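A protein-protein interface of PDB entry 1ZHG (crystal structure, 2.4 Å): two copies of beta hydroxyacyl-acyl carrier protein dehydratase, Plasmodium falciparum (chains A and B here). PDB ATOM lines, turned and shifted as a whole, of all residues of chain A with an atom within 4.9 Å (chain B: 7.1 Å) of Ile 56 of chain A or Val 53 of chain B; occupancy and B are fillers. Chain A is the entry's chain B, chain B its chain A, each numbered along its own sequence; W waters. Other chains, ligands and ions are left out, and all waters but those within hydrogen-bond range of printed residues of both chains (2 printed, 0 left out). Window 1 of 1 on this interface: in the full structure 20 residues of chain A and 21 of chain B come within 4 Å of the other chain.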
ATOM      1  N   GLY A  52     -29.496   2.837 -12.872  1.00  0.00           N
ATOM      2  CA  GLY A  52     -29.384   4.195 -13.367  1.00  0.00           C
ATOM      3  C   GLY A  52     -29.132   4.254 -14.866  1.00  0.00           C
ATOM      4  O   GLY A  52     -29.755   5.047 -15.572  1.00  0.00           O
ATOM      5  N   VAL A  53     -28.237   3.408 -15.365  1.00  0.00           N
ATOM      6  CA  VAL A  53     -27.925   3.412 -16.788  1.00  0.00           C
ATOM      7  C   VAL A  53     -29.130   3.150 -17.693  1.00  0.00           C
ATOM      8  O   VAL A  53     -29.139   3.577 -18.850  1.00  0.00           O
ATOM      9  CB  VAL A  53     -26.798   2.395 -17.137  1.00  0.00           C
ATOM     10  CG1 VAL A  53     -25.496   2.797 -16.456  1.00  0.00           C
ATOM     11  CG2 VAL A  53     -27.216   1.001 -16.733  1.00  0.00           C
ATOM     12  N   LEU A  54     -30.140   2.449 -17.183  1.00  0.00           N
ATOM     13  CA  LEU A  54     -31.325   2.189 -17.993  1.00  0.00           C
ATOM     14  C   LEU A  54     -32.253   3.399 -17.940  1.00  0.00           C
ATOM     15  O   LEU A  54     -33.093   3.580 -18.817  1.00  0.00           O
ATOM     16  CB  LEU A  54     -32.054   0.926 -17.517  1.00  0.00           C
ATOM     17  CG  LEU A  54     -31.244  -0.371 -17.652  1.00  0.00           C
ATOM     18  CD1 LEU A  54     -32.098  -1.543 -17.219  1.00  0.00           C
ATOM     19  CD2 LEU A  54     -30.767  -0.564 -19.082  1.00  0.00           C
ATOM     20  N   GLN A  55     -32.110   4.218 -16.901  1.00  0.00           N
ATOM     21  CA  GLN A  55     -32.913   5.427 -16.782  1.00  0.00           C
ATOM     22  C   GLN A  55     -32.410   6.330 -17.904  1.00  0.00           C
ATOM     23  O   GLN A  55     -33.180   7.046 -18.537  1.00  0.00           O
ATOM     24  CB  GLN A  55     -32.712   6.076 -15.405  1.00  0.00           C
ATOM     25  CG  GLN A  55     -33.484   5.376 -14.290  1.00  0.00           C
ATOM     26  CD  GLN A  55     -33.151   5.905 -12.916  1.00  0.00           C
ATOM     27  OE1 GLN A  55     -33.190   7.108 -12.681  1.00  0.00           O
ATOM     28  NE2 GLN A  55     -32.826   5.003 -11.992  1.00  0.00           N
ATOM     29  N   ILE A  56     -31.104   6.268 -18.147  1.00  0.00           N
ATOM     30  CA  ILE A  56     -30.480   7.017 -19.228  1.00  0.00           C
ATOM     31  C   ILE A  56     -31.047   6.505 -20.549  1.00  0.00           C
ATOM     32  O   ILE A  56     -31.416   7.285 -21.422  1.00  0.00           O
ATOM     33  CB  ILE A  56     -28.963   6.790 -19.263  1.00  0.00           C
ATOM     34  CG1 ILE A  56     -28.310   7.456 -18.056  1.00  0.00           C
ATOM     35  CG2 ILE A  56     -28.388   7.306 -20.570  1.00  0.00           C
ATOM     36  CD1 ILE A  56     -26.831   7.232 -17.999  1.00  0.00           C
ATOM     37  N   GLU A  57     -31.114   5.185 -20.687  1.00  0.00           N
ATOM     38  CA  GLU A  57     -31.625   4.568 -21.902  1.00  0.00           C
ATOM     39  C   GLU A  57     -33.063   5.004 -22.186  1.00  0.00           C
ATOM     40  O   GLU A  57     -33.411   5.310 -23.325  1.00  0.00           O
ATOM     41  CB  GLU A  57     -31.541   3.033 -21.788  1.00  0.00           C
ATOM     42  CG  GLU A  57     -32.083   2.258 -22.995  1.00  0.00           C
ATOM     43  CD  GLU A  57     -31.271   2.465 -24.264  1.00  0.00           C
ATOM     44  OE1 GLU A  57     -31.818   2.249 -25.362  1.00  0.00           O
ATOM     45  OE2 GLU A  57     -30.083   2.831 -24.182  1.00  0.00           O
ATOM     46  N   ALA A  58     -33.889   5.042 -21.145  1.00  0.00           N
ATOM     47  CA  ALA A  58     -35.290   5.425 -21.298  1.00  0.00           C
ATOM     48  C   ALA A  58     -35.395   6.865 -21.758  1.00  0.00           C
ATOM     49  O   ALA A  58     -36.209   7.196 -22.612  1.00  0.00           O
ATOM     50  CB  ALA A  58     -36.036   5.239 -19.983  1.00  0.00           C
ATOM     51  N   LEU A  59     -34.567   7.724 -21.184  1.00  0.00           N
ATOM     52  CA  LEU A  59     -34.579   9.123 -21.565  1.00  0.00           C
ATOM     53  C   LEU A  59     -34.090   9.289 -22.998  1.00  0.00           C
ATOM     54  O   LEU A  59     -34.614  10.119 -23.743  1.00  0.00           O
ATOM     55  CB  LEU A  59     -33.735   9.955 -20.586  1.00  0.00           C
ATOM     56  CG  LEU A  59     -34.617  10.524 -19.460  1.00  0.00           C
ATOM     57  CD1 LEU A  59     -33.793  11.025 -18.280  1.00  0.00           C
ATOM     58  CD2 LEU A  59     -35.475  11.643 -20.042  1.00  0.00           C
ATOM     59  N   ALA A  60     -33.117   8.469 -23.385  1.00  0.00           N
ATOM     60  CA  ALA A  60     -32.551   8.534 -24.725  1.00  0.00           C
ATOM     61  C   ALA A  60     -33.551   8.088 -25.779  1.00  0.00           C
ATOM     62  O   ALA A  60     -33.613   8.663 -26.866  1.00  0.00           O
ATOM     63  CB  ALA A  60     -31.284   7.686 -24.801  1.00  0.00           C
ATOM     64  N   PHE A  81     -27.424   7.095 -30.796  1.00  0.00           N
ATOM     65  CA  PHE A  81     -27.059   7.687 -29.508  1.00  0.00           C
ATOM     66  C   PHE A  81     -25.534   7.732 -29.495  1.00  0.00           C
ATOM     67  O   PHE A  81     -24.889   6.693 -29.349  1.00  0.00           O
ATOM     68  CB  PHE A  81     -27.579   6.783 -28.386  1.00  0.00           C
ATOM     69  CG  PHE A  81     -27.621   7.434 -27.033  1.00  0.00           C
ATOM     70  CD1 PHE A  81     -27.824   6.661 -25.893  1.00  0.00           C
ATOM     71  CD2 PHE A  81     -27.469   8.810 -26.893  1.00  0.00           C
ATOM     72  CE1 PHE A  81     -27.874   7.243 -24.642  1.00  0.00           C
ATOM     73  CE2 PHE A  81     -27.516   9.401 -25.643  1.00  0.00           C
ATOM     74  CZ  PHE A  81     -27.718   8.620 -24.515  1.00  0.00           C
ATOM     75  N   VAL A  84     -23.443  11.371 -24.126  1.00  0.00           N
ATOM     76  CA  VAL A  84     -24.315  11.840 -23.067  1.00  0.00           C
ATOM     77  C   VAL A  84     -23.444  12.500 -21.994  1.00  0.00           C
ATOM     78  O   VAL A  84     -22.362  12.014 -21.683  1.00  0.00           O
ATOM     79  CB  VAL A  84     -25.146  10.665 -22.460  1.00  0.00           C
ATOM     80  CG1 VAL A  84     -24.242   9.687 -21.716  1.00  0.00           C
ATOM     81  CG2 VAL A  84     -26.215  11.213 -21.524  1.00  0.00           C
ATOM     82  N   VAL A  87     -25.137  13.554 -16.268  1.00  0.00           N
ATOM     83  CA  VAL A  87     -26.235  12.764 -15.736  1.00  0.00           C
ATOM     84  C   VAL A  87     -26.052  12.648 -14.230  1.00  0.00           C
ATOM     85  O   VAL A  87     -24.952  12.388 -13.736  1.00  0.00           O
ATOM     86  CB  VAL A  87     -26.346  11.343 -16.400  1.00  0.00           C
ATOM     87  CG1 VAL A  87     -25.528  11.289 -17.654  1.00  0.00           C
ATOM     88  CG2 VAL A  87     -25.941  10.255 -15.433  1.00  0.00           C
ATOM     89  N   TRP A  89     -27.979  10.930 -10.768  1.00  0.00           N
ATOM     90  CA  TRP A  89     -29.002  10.042 -10.213  1.00  0.00           C
ATOM     91  C   TRP A  89     -29.264  10.438  -8.771  1.00  0.00           C
ATOM     92  O   TRP A  89     -28.423  10.215  -7.908  1.00  0.00           O
ATOM     93  CB  TRP A  89     -28.536   8.586 -10.256  1.00  0.00           C
ATOM     94  CG  TRP A  89     -28.478   8.024 -11.622  1.00  0.00           C
ATOM     95  CD1 TRP A  89     -29.532   7.773 -12.448  1.00  0.00           C
ATOM     96  CD2 TRP A  89     -27.299   7.661 -12.347  1.00  0.00           C
ATOM     97  NE1 TRP A  89     -29.084   7.277 -13.649  1.00  0.00           N
ATOM     98  CE2 TRP A  89     -27.720   7.201 -13.616  1.00  0.00           C
ATOM     99  CE3 TRP A  89     -25.935   7.689 -12.056  1.00  0.00           C
ATOM    100  CZ2 TRP A  89     -26.813   6.757 -14.588  1.00  0.00           C
ATOM    101  CZ3 TRP A  89     -25.037   7.250 -13.023  1.00  0.00           C
ATOM    102  CH2 TRP A  89     -25.482   6.795 -14.276  1.00  0.00           C
ATOM    103  N   ILE A 129     -33.605  11.806 -11.633  1.00  0.00           N
ATOM    104  CA  ILE A 129     -32.455  11.872 -12.525  1.00  0.00           C
ATOM    105  C   ILE A 129     -32.502  13.070 -13.470  1.00  0.00           C
ATOM    106  O   ILE A 129     -33.560  13.413 -14.000  1.00  0.00           O
ATOM    107  CB  ILE A 129     -32.320  10.601 -13.392  1.00  0.00           C
ATOM    108  CG1 ILE A 129     -31.175  10.795 -14.398  1.00  0.00           C
ATOM    109  CG2 ILE A 129     -33.633  10.303 -14.102  1.00  0.00           C
ATOM    110  CD1 ILE A 129     -30.942   9.637 -15.342  1.00  0.00           C
ATOM    111  N   ILE A 131     -30.347  14.910 -16.828  1.00  0.00           N
ATOM    112  CA  ILE A 131     -29.371  14.679 -17.872  1.00  0.00           C
ATOM    113  C   ILE A 131     -29.214  15.980 -18.635  1.00  0.00           C
ATOM    114  O   ILE A 131     -30.115  16.404 -19.355  1.00  0.00           O
ATOM    115  CB  ILE A 131     -29.792  13.558 -18.857  1.00  0.00           C
ATOM    116  CG1 ILE A 131     -29.892  12.216 -18.131  1.00  0.00           C
ATOM    117  CG2 ILE A 131     -28.744  13.427 -19.964  1.00  0.00           C
ATOM    118  CD1 ILE A 131     -30.259  11.051 -19.039  1.00  0.00           C
ATOM    119  N   MET A 134     -27.814  14.968 -24.213  1.00  0.00           N
ATOM    120  CA  MET A 134     -27.744  13.676 -24.894  1.00  0.00           C
ATOM    121  C   MET A 134     -27.494  14.049 -26.351  1.00  0.00           C
ATOM    122  O   MET A 134     -28.189  14.909 -26.892  1.00  0.00           O
ATOM    123  CB  MET A 134     -29.072  12.917 -24.796  1.00  0.00           C
ATOM    124  CG  MET A 134     -29.405  12.354 -23.433  1.00  0.00           C
ATOM    125  SD  MET A 134     -31.104  11.735 -23.379  1.00  0.00           S
ATOM    126  CE  MET A 134     -32.009  13.230 -22.969  1.00  0.00           C
ATOM    127  N   TYR B  10     -26.696  -2.966 -10.976  1.00  0.00           N
ATOM    128  CA  TYR B  10     -27.136  -3.554 -12.239  1.00  0.00           C
ATOM    129  C   TYR B  10     -26.935  -5.025 -11.894  1.00  0.00           C
ATOM    130  O   TYR B  10     -25.896  -5.405 -11.367  1.00  0.00           O
ATOM    131  CB  TYR B  10     -26.236  -3.149 -13.411  1.00  0.00           C
ATOM    132  CG  TYR B  10     -26.684  -3.730 -14.745  1.00  0.00           C
ATOM    133  CD1 TYR B  10     -27.896  -3.353 -15.324  1.00  0.00           C
ATOM    134  CD2 TYR B  10     -25.916  -4.694 -15.401  1.00  0.00           C
ATOM    135  CE1 TYR B  10     -28.335  -3.926 -16.520  1.00  0.00           C
ATOM    136  CE2 TYR B  10     -26.346  -5.270 -16.595  1.00  0.00           C
ATOM    137  CZ  TYR B  10     -27.556  -4.885 -17.146  1.00  0.00           C
ATOM    138  OH  TYR B  10     -28.001  -5.482 -18.305  1.00  0.00           O
ATOM    139  N   LEU B  14     -20.470  -7.016 -15.432  1.00  0.00           N
ATOM    140  CA  LEU B  14     -19.996  -6.861 -16.798  1.00  0.00           C
ATOM    141  C   LEU B  14     -18.474  -6.775 -16.912  1.00  0.00           C
ATOM    142  O   LEU B  14     -17.940  -6.126 -17.814  1.00  0.00           O
ATOM    143  CB  LEU B  14     -20.638  -5.627 -17.424  1.00  0.00           C
ATOM    144  CG  LEU B  14     -22.166  -5.570 -17.450  1.00  0.00           C
ATOM    145  CD1 LEU B  14     -22.603  -4.279 -18.135  1.00  0.00           C
ATOM    146  CD2 LEU B  14     -22.727  -6.771 -18.180  1.00  0.00           C
ATOM    147  N   MET B  50     -23.791  -4.407 -28.593  1.00  0.00           N
ATOM    148  CA  MET B  50     -23.856  -4.047 -27.178  1.00  0.00           C
ATOM    149  C   MET B  50     -24.264  -2.588 -27.000  1.00  0.00           C
ATOM    150  O   MET B  50     -23.692  -1.694 -27.617  1.00  0.00           O
ATOM    151  CB  MET B  50     -22.506  -4.313 -26.502  1.00  0.00           C
ATOM    152  CG  MET B  50     -22.479  -4.007 -25.025  1.00  0.00           C
ATOM    153  SD  MET B  50     -20.912  -4.497 -24.270  1.00  0.00           S
ATOM    154  CE  MET B  50     -21.271  -4.242 -22.533  1.00  0.00           C
ATOM    155  N   PRO B  51     -25.280  -2.335 -26.156  1.00  0.00           N
ATOM    156  CA  PRO B  51     -25.780  -0.981 -25.894  1.00  0.00           C
ATOM    157  C   PRO B  51     -24.732  -0.147 -25.179  1.00  0.00           C
ATOM    158  O   PRO B  51     -24.145  -0.600 -24.191  1.00  0.00           O
ATOM    159  CB  PRO B  51     -27.006  -1.230 -25.017  1.00  0.00           C
ATOM    160  CG  PRO B  51     -27.427  -2.601 -25.387  1.00  0.00           C
ATOM    161  CD  PRO B  51     -26.120  -3.326 -25.461  1.00  0.00           C
ATOM    162  N   GLY B  52     -24.513   1.071 -25.676  1.00  0.00           N
ATOM    163  CA  GLY B  52     -23.522   1.947 -25.080  1.00  0.00           C
ATOM    164  C   GLY B  52     -23.744   2.147 -23.596  1.00  0.00           C
ATOM    165  O   GLY B  52     -22.805   2.276 -22.812  1.00  0.00           O
ATOM    166  N   VAL B  53     -25.008   2.183 -23.212  1.00  0.00           N
ATOM    167  CA  VAL B  53     -25.385   2.377 -21.828  1.00  0.00           C
ATOM    168  C   VAL B  53     -24.788   1.304 -20.926  1.00  0.00           C
ATOM    169  O   VAL B  53     -24.363   1.597 -19.804  1.00  0.00           O
ATOM    170  CB  VAL B  53     -26.935   2.406 -21.705  1.00  0.00           C
ATOM    171  CG1 VAL B  53     -27.388   1.798 -20.396  1.00  0.00           C
ATOM    172  CG2 VAL B  53     -27.415   3.843 -21.814  1.00  0.00           C
ATOM    173  N   LEU B  54     -24.743   0.068 -21.417  1.00  0.00           N
ATOM    174  CA  LEU B  54     -24.193  -1.012 -20.626  1.00  0.00           C
ATOM    175  C   LEU B  54     -22.676  -0.971 -20.644  1.00  0.00           C
ATOM    176  O   LEU B  54     -22.029  -1.600 -19.818  1.00  0.00           O
ATOM    177  CB  LEU B  54     -24.732  -2.353 -21.115  1.00  0.00           C
ATOM    178  CG  LEU B  54     -26.255  -2.461 -20.924  1.00  0.00           C
ATOM    179  CD1 LEU B  54     -26.729  -3.782 -21.413  1.00  0.00           C
ATOM    180  CD2 LEU B  54     -26.628  -2.286 -19.454  1.00  0.00           C
ATOM    181  N   GLN B  55     -22.115  -0.206 -21.577  1.00  0.00           N
ATOM    182  CA  GLN B  55     -20.670  -0.046 -21.664  1.00  0.00           C
ATOM    183  C   GLN B  55     -20.297   0.904 -20.537  1.00  0.00           C
ATOM    184  O   GLN B  55     -19.230   0.796 -19.938  1.00  0.00           O
ATOM    185  CB  GLN B  55     -20.257   0.533 -23.023  1.00  0.00           C
ATOM    186  CG  GLN B  55     -20.241  -0.482 -24.167  1.00  0.00           C
ATOM    187  CD  GLN B  55     -20.052   0.167 -25.547  1.00  0.00           C
ATOM    188  OE1 GLN B  55     -19.173   1.000 -25.749  1.00  0.00           O
ATOM    189  NE2 GLN B  55     -20.876  -0.230 -26.494  1.00  0.00           N
ATOM    190  N   ILE B  56     -21.198   1.835 -20.247  1.00  0.00           N
ATOM    191  CA  ILE B  56     -21.004   2.784 -19.163  1.00  0.00           C
ATOM    192  C   ILE B  56     -21.004   1.996 -17.857  1.00  0.00           C
ATOM    193  O   ILE B  56     -20.148   2.187 -16.996  1.00  0.00           O
ATOM    194  CB  ILE B  56     -22.159   3.820 -19.123  1.00  0.00           C
ATOM    195  CG1 ILE B  56     -22.048   4.760 -20.326  1.00  0.00           C
ATOM    196  CG2 ILE B  56     -22.144   4.601 -17.799  1.00  0.00           C
ATOM    197  CD1 ILE B  56     -23.193   5.758 -20.434  1.00  0.00           C
ATOM    198  N   GLU B  57     -21.985   1.108 -17.733  1.00  0.00           N
ATOM    199  CA  GLU B  57     -22.164   0.266 -16.565  1.00  0.00           C
ATOM    200  C   GLU B  57     -20.951  -0.609 -16.335  1.00  0.00           C
ATOM    201  O   GLU B  57     -20.550  -0.829 -15.201  1.00  0.00           O
ATOM    202  CB  GLU B  57     -23.407  -0.608 -16.755  1.00  0.00           C
ATOM    203  CG  GLU B  57     -23.635  -1.640 -15.653  1.00  0.00           C
ATOM    204  CD  GLU B  57     -23.955  -1.006 -14.317  1.00  0.00           C
ATOM    205  OE1 GLU B  57     -23.705  -1.650 -13.276  1.00  0.00           O
ATOM    206  OE2 GLU B  57     -24.466   0.131 -14.304  1.00  0.00           O
ATOM    207  N   ALA B  58     -20.377  -1.115 -17.425  1.00  0.00           N
ATOM    208  CA  ALA B  58     -19.205  -1.977 -17.357  1.00  0.00           C
ATOM    209  C   ALA B  58     -18.046  -1.206 -16.748  1.00  0.00           C
ATOM    210  O   ALA B  58     -17.371  -1.690 -15.843  1.00  0.00           O
ATOM    211  CB  ALA B  58     -18.835  -2.452 -18.747  1.00  0.00           C
ATOM    212  N   PHE B  81     -23.175   4.664  -7.549  1.00  0.00           N
ATOM    213  CA  PHE B  81     -22.954   5.334  -8.826  1.00  0.00           C
ATOM    214  C   PHE B  81     -23.934   6.496  -8.859  1.00  0.00           C
ATOM    215  O   PHE B  81     -25.137   6.290  -9.001  1.00  0.00           O
ATOM    216  CB  PHE B  81     -23.217   4.345  -9.964  1.00  0.00           C
ATOM    217  CG  PHE B  81     -22.746   4.812 -11.307  1.00  0.00           C
ATOM    218  CD1 PHE B  81     -21.757   5.787 -11.422  1.00  0.00           C
ATOM    219  CD2 PHE B  81     -23.264   4.244 -12.467  1.00  0.00           C
ATOM    220  CE1 PHE B  81     -21.296   6.185 -12.673  1.00  0.00           C
ATOM    221  CE2 PHE B  81     -22.807   4.637 -13.722  1.00  0.00           C
ATOM    222  CZ  PHE B  81     -21.820   5.608 -13.826  1.00  0.00           C
ATOM    223  N   VAL B  84     -22.453  10.598 -14.248  1.00  0.00           N
ATOM    224  CA  VAL B  84     -21.474  10.359 -15.300  1.00  0.00           C
ATOM    225  C   VAL B  84     -21.461  11.506 -16.313  1.00  0.00           C
ATOM    226  O   VAL B  84     -22.513  11.945 -16.773  1.00  0.00           O
ATOM    227  CB  VAL B  84     -21.735   9.012 -16.029  1.00  0.00           C
ATOM    228  CG1 VAL B  84     -23.047   9.055 -16.768  1.00  0.00           C
ATOM    229  CG2 VAL B  84     -20.602   8.723 -16.987  1.00  0.00           C
ATOM    230  N   VAL B  87     -19.531  11.249 -21.896  1.00  0.00           N
ATOM    231  CA  VAL B  87     -19.523   9.885 -22.391  1.00  0.00           C
ATOM    232  C   VAL B  87     -19.581   9.952 -23.910  1.00  0.00           C
ATOM    233  O   VAL B  87     -20.480  10.576 -24.473  1.00  0.00           O
ATOM    234  CB  VAL B  87     -20.749   9.074 -21.879  1.00  0.00           C
ATOM    235  CG1 VAL B  87     -20.743   7.699 -22.484  1.00  0.00           C
ATOM    236  CG2 VAL B  87     -20.730   8.982 -20.367  1.00  0.00           C
ATOM    237  N   TRP B  89     -19.365   7.445 -27.376  1.00  0.00           N
ATOM    238  CA  TRP B  89     -19.317   6.118 -27.969  1.00  0.00           C
ATOM    239  C   TRP B  89     -18.675   6.258 -29.344  1.00  0.00           C
ATOM    240  O   TRP B  89     -19.237   6.881 -30.240  1.00  0.00           O
ATOM    241  CB  TRP B  89     -20.732   5.552 -28.081  1.00  0.00           C
ATOM    242  CG  TRP B  89     -21.340   5.236 -26.740  1.00  0.00           C
ATOM    243  CD1 TRP B  89     -20.962   4.239 -25.889  1.00  0.00           C
ATOM    244  CD2 TRP B  89     -22.436   5.916 -26.103  1.00  0.00           C
ATOM    245  NE1 TRP B  89     -21.757   4.248 -24.768  1.00  0.00           N
ATOM    246  CE2 TRP B  89     -22.672   5.260 -24.873  1.00  0.00           C
ATOM    247  CE3 TRP B  89     -23.247   7.002 -26.457  1.00  0.00           C
ATOM    248  CZ2 TRP B  89     -23.683   5.664 -23.989  1.00  0.00           C
ATOM    249  CZ3 TRP B  89     -24.256   7.404 -25.578  1.00  0.00           C
ATOM    250  CH2 TRP B  89     -24.466   6.730 -24.359  1.00  0.00           C
ATOM    251  N   ILE B 129     -15.049   3.616 -26.530  1.00  0.00           N
ATOM    252  CA  ILE B 129     -15.795   4.465 -25.617  1.00  0.00           C
ATOM    253  C   ILE B 129     -14.884   5.280 -24.698  1.00  0.00           C
ATOM    254  O   ILE B 129     -13.835   4.810 -24.259  1.00  0.00           O
ATOM    255  CB  ILE B 129     -16.789   3.661 -24.735  1.00  0.00           C
ATOM    256  CG1 ILE B 129     -17.597   4.637 -23.869  1.00  0.00           C
ATOM    257  CG2 ILE B 129     -16.046   2.652 -23.866  1.00  0.00           C
ATOM    258  CD1 ILE B 129     -18.633   3.999 -22.970  1.00  0.00           C
HETATM  259  O   HOH W   1     -27.578   2.323 -25.111  1.00  0.00           O
HETATM  260  O   HOH W   2     -26.882   1.440 -13.500  1.00  0.00           O
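The backbone carbonyl oxygen (O) of Val 87 of chain A is in hydrogen-bond range of the backbone NH (N) of Val 84 of chain B, 3.1 Å away. The backbone NH of Val 87 of chain B lies within hydrogen-bond range of the backbone carbonyl oxygen of Val 84 of chain A (2.9 Å).
O of Gly 52 of chain A lies within hydrogen-bond range of NE1 of Trp 89 of chain A. O of Gly 52 of chain B sits close to NE1 of Trp 89 of chain B, 3.0 Å away.
O of Val 53 of chain A touches CG1 of Val 53 of chain B, 2.9 Å away. OE2 of Glu 57 of chain B touches CG1 of Val 53 of chain A, 3.6 Å away. CG2 of Val 53 of chain B touches CG2 of Ile 56 of chain A (3.8 Å). OE2 of Glu 57 of chain A touches CG2 of Val 53 of chain B, at 3.7 Å. O of Phe 81 of chain A touches CE3 of Trp 89 of chain B (3.3 Å). Val 84 of chain A touches Trp 89 of chain B. CE3 of Trp 89 of chain A touches O of Phe 81 of chain B, at 3.5 Å.
Printed residues of chain B within 4 Å of Ile 56 of chain A: Val 53. Of the printed residues of chain B, Glu 57 of chain A touches Val 53. Of the printed residues of chain B, Phe 81 of chain A touches Trp 89. Met 134 of chain A touches none of the printed residues of chain B. Val 53 of chain B touches just these residues of chain A: Val 53 (2.9 Å), Ile 56 (3.8 Å) and Glu 57 (3.7 Å). Gln 55 of chain B touches none of the printed residues of chain A. Of the printed residues of chain A, Val 87 of chain B touches Val 84 (2.9 Å). Of the printed residues of chain A, Trp 89 of chain B touches Phe 81 (3.3 Å) and Val 84 (3.97 Å). The nearest residue of chain B that does not touch Ile 56 of chain A is Val 84 of chain B (4.4 Å). The nearest residue of chain A that does not touch Val 53 of chain B is Leu 54 of chain A (4.3 Å). The nearest printed residue of chain A that does not touch Val 84 of chain B is Trp 89 of chain A (4.2 Å).
Of the 16 printed residues of chain B, 6 touch a printed residue of chain A. Printed residues of chain B that touch a printed residue of chain A: Val 53, Glu 57, Phe 81, Val 84, Val 87 and Trp 89. Hydrophobic or aromatic side chains of chain B that line the printed part of chain A: Val 53, Phe 81, Val 84, Val 87 and Trp 89. Of the 16 printed residues of chain A, 7 touch a printed residue of chain B. Hydrophobic or aromatic side chains of chain A within 4 Å of the printed part of chain B: Val 53, Ile 56, Phe 81, Val 84, Val 87 and Trp 89. Among the printed residues, 9 pairs touch across the chains. Among the printed residues, no Asp or Glu carboxylate lies within 4 Å of a Lys or Arg side-chain nitrogen of the other chain.
Val 53 of chain A touches its own counterpart, Val 53 of chain B. Val 53 of chain A touches Glu 57 of chain B, and with the chains exchanged Glu 57 of chain A touches Val 53 of chain B. Ile 56 of chain A touches Val 53 of chain B, but with the chains exchanged Val 53 of chain A does not touch Ile 56 of chain B (4.04 Å). Phe 81 of chain A touches Trp 89 of chain B, and with the chains exchanged Trp 89 of chain A touches Phe 81 of chain B. 12 positions are printed for both chains.
Water W1 lies within hydrogen-bond range of OE2 of Glu 57 of chain A, N of Val 53 of chain B and N of Gly 52 of chain B. Water W2 lies within hydrogen-bond range of the side-chain carboxylate (OE2) of Glu 57 of chain B (2.9 Å), the backbone NH (N) of Gly 52 of chain A (3.0 Å) and the backbone NH (N) of Val 53 of chain A (3.0 Å).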
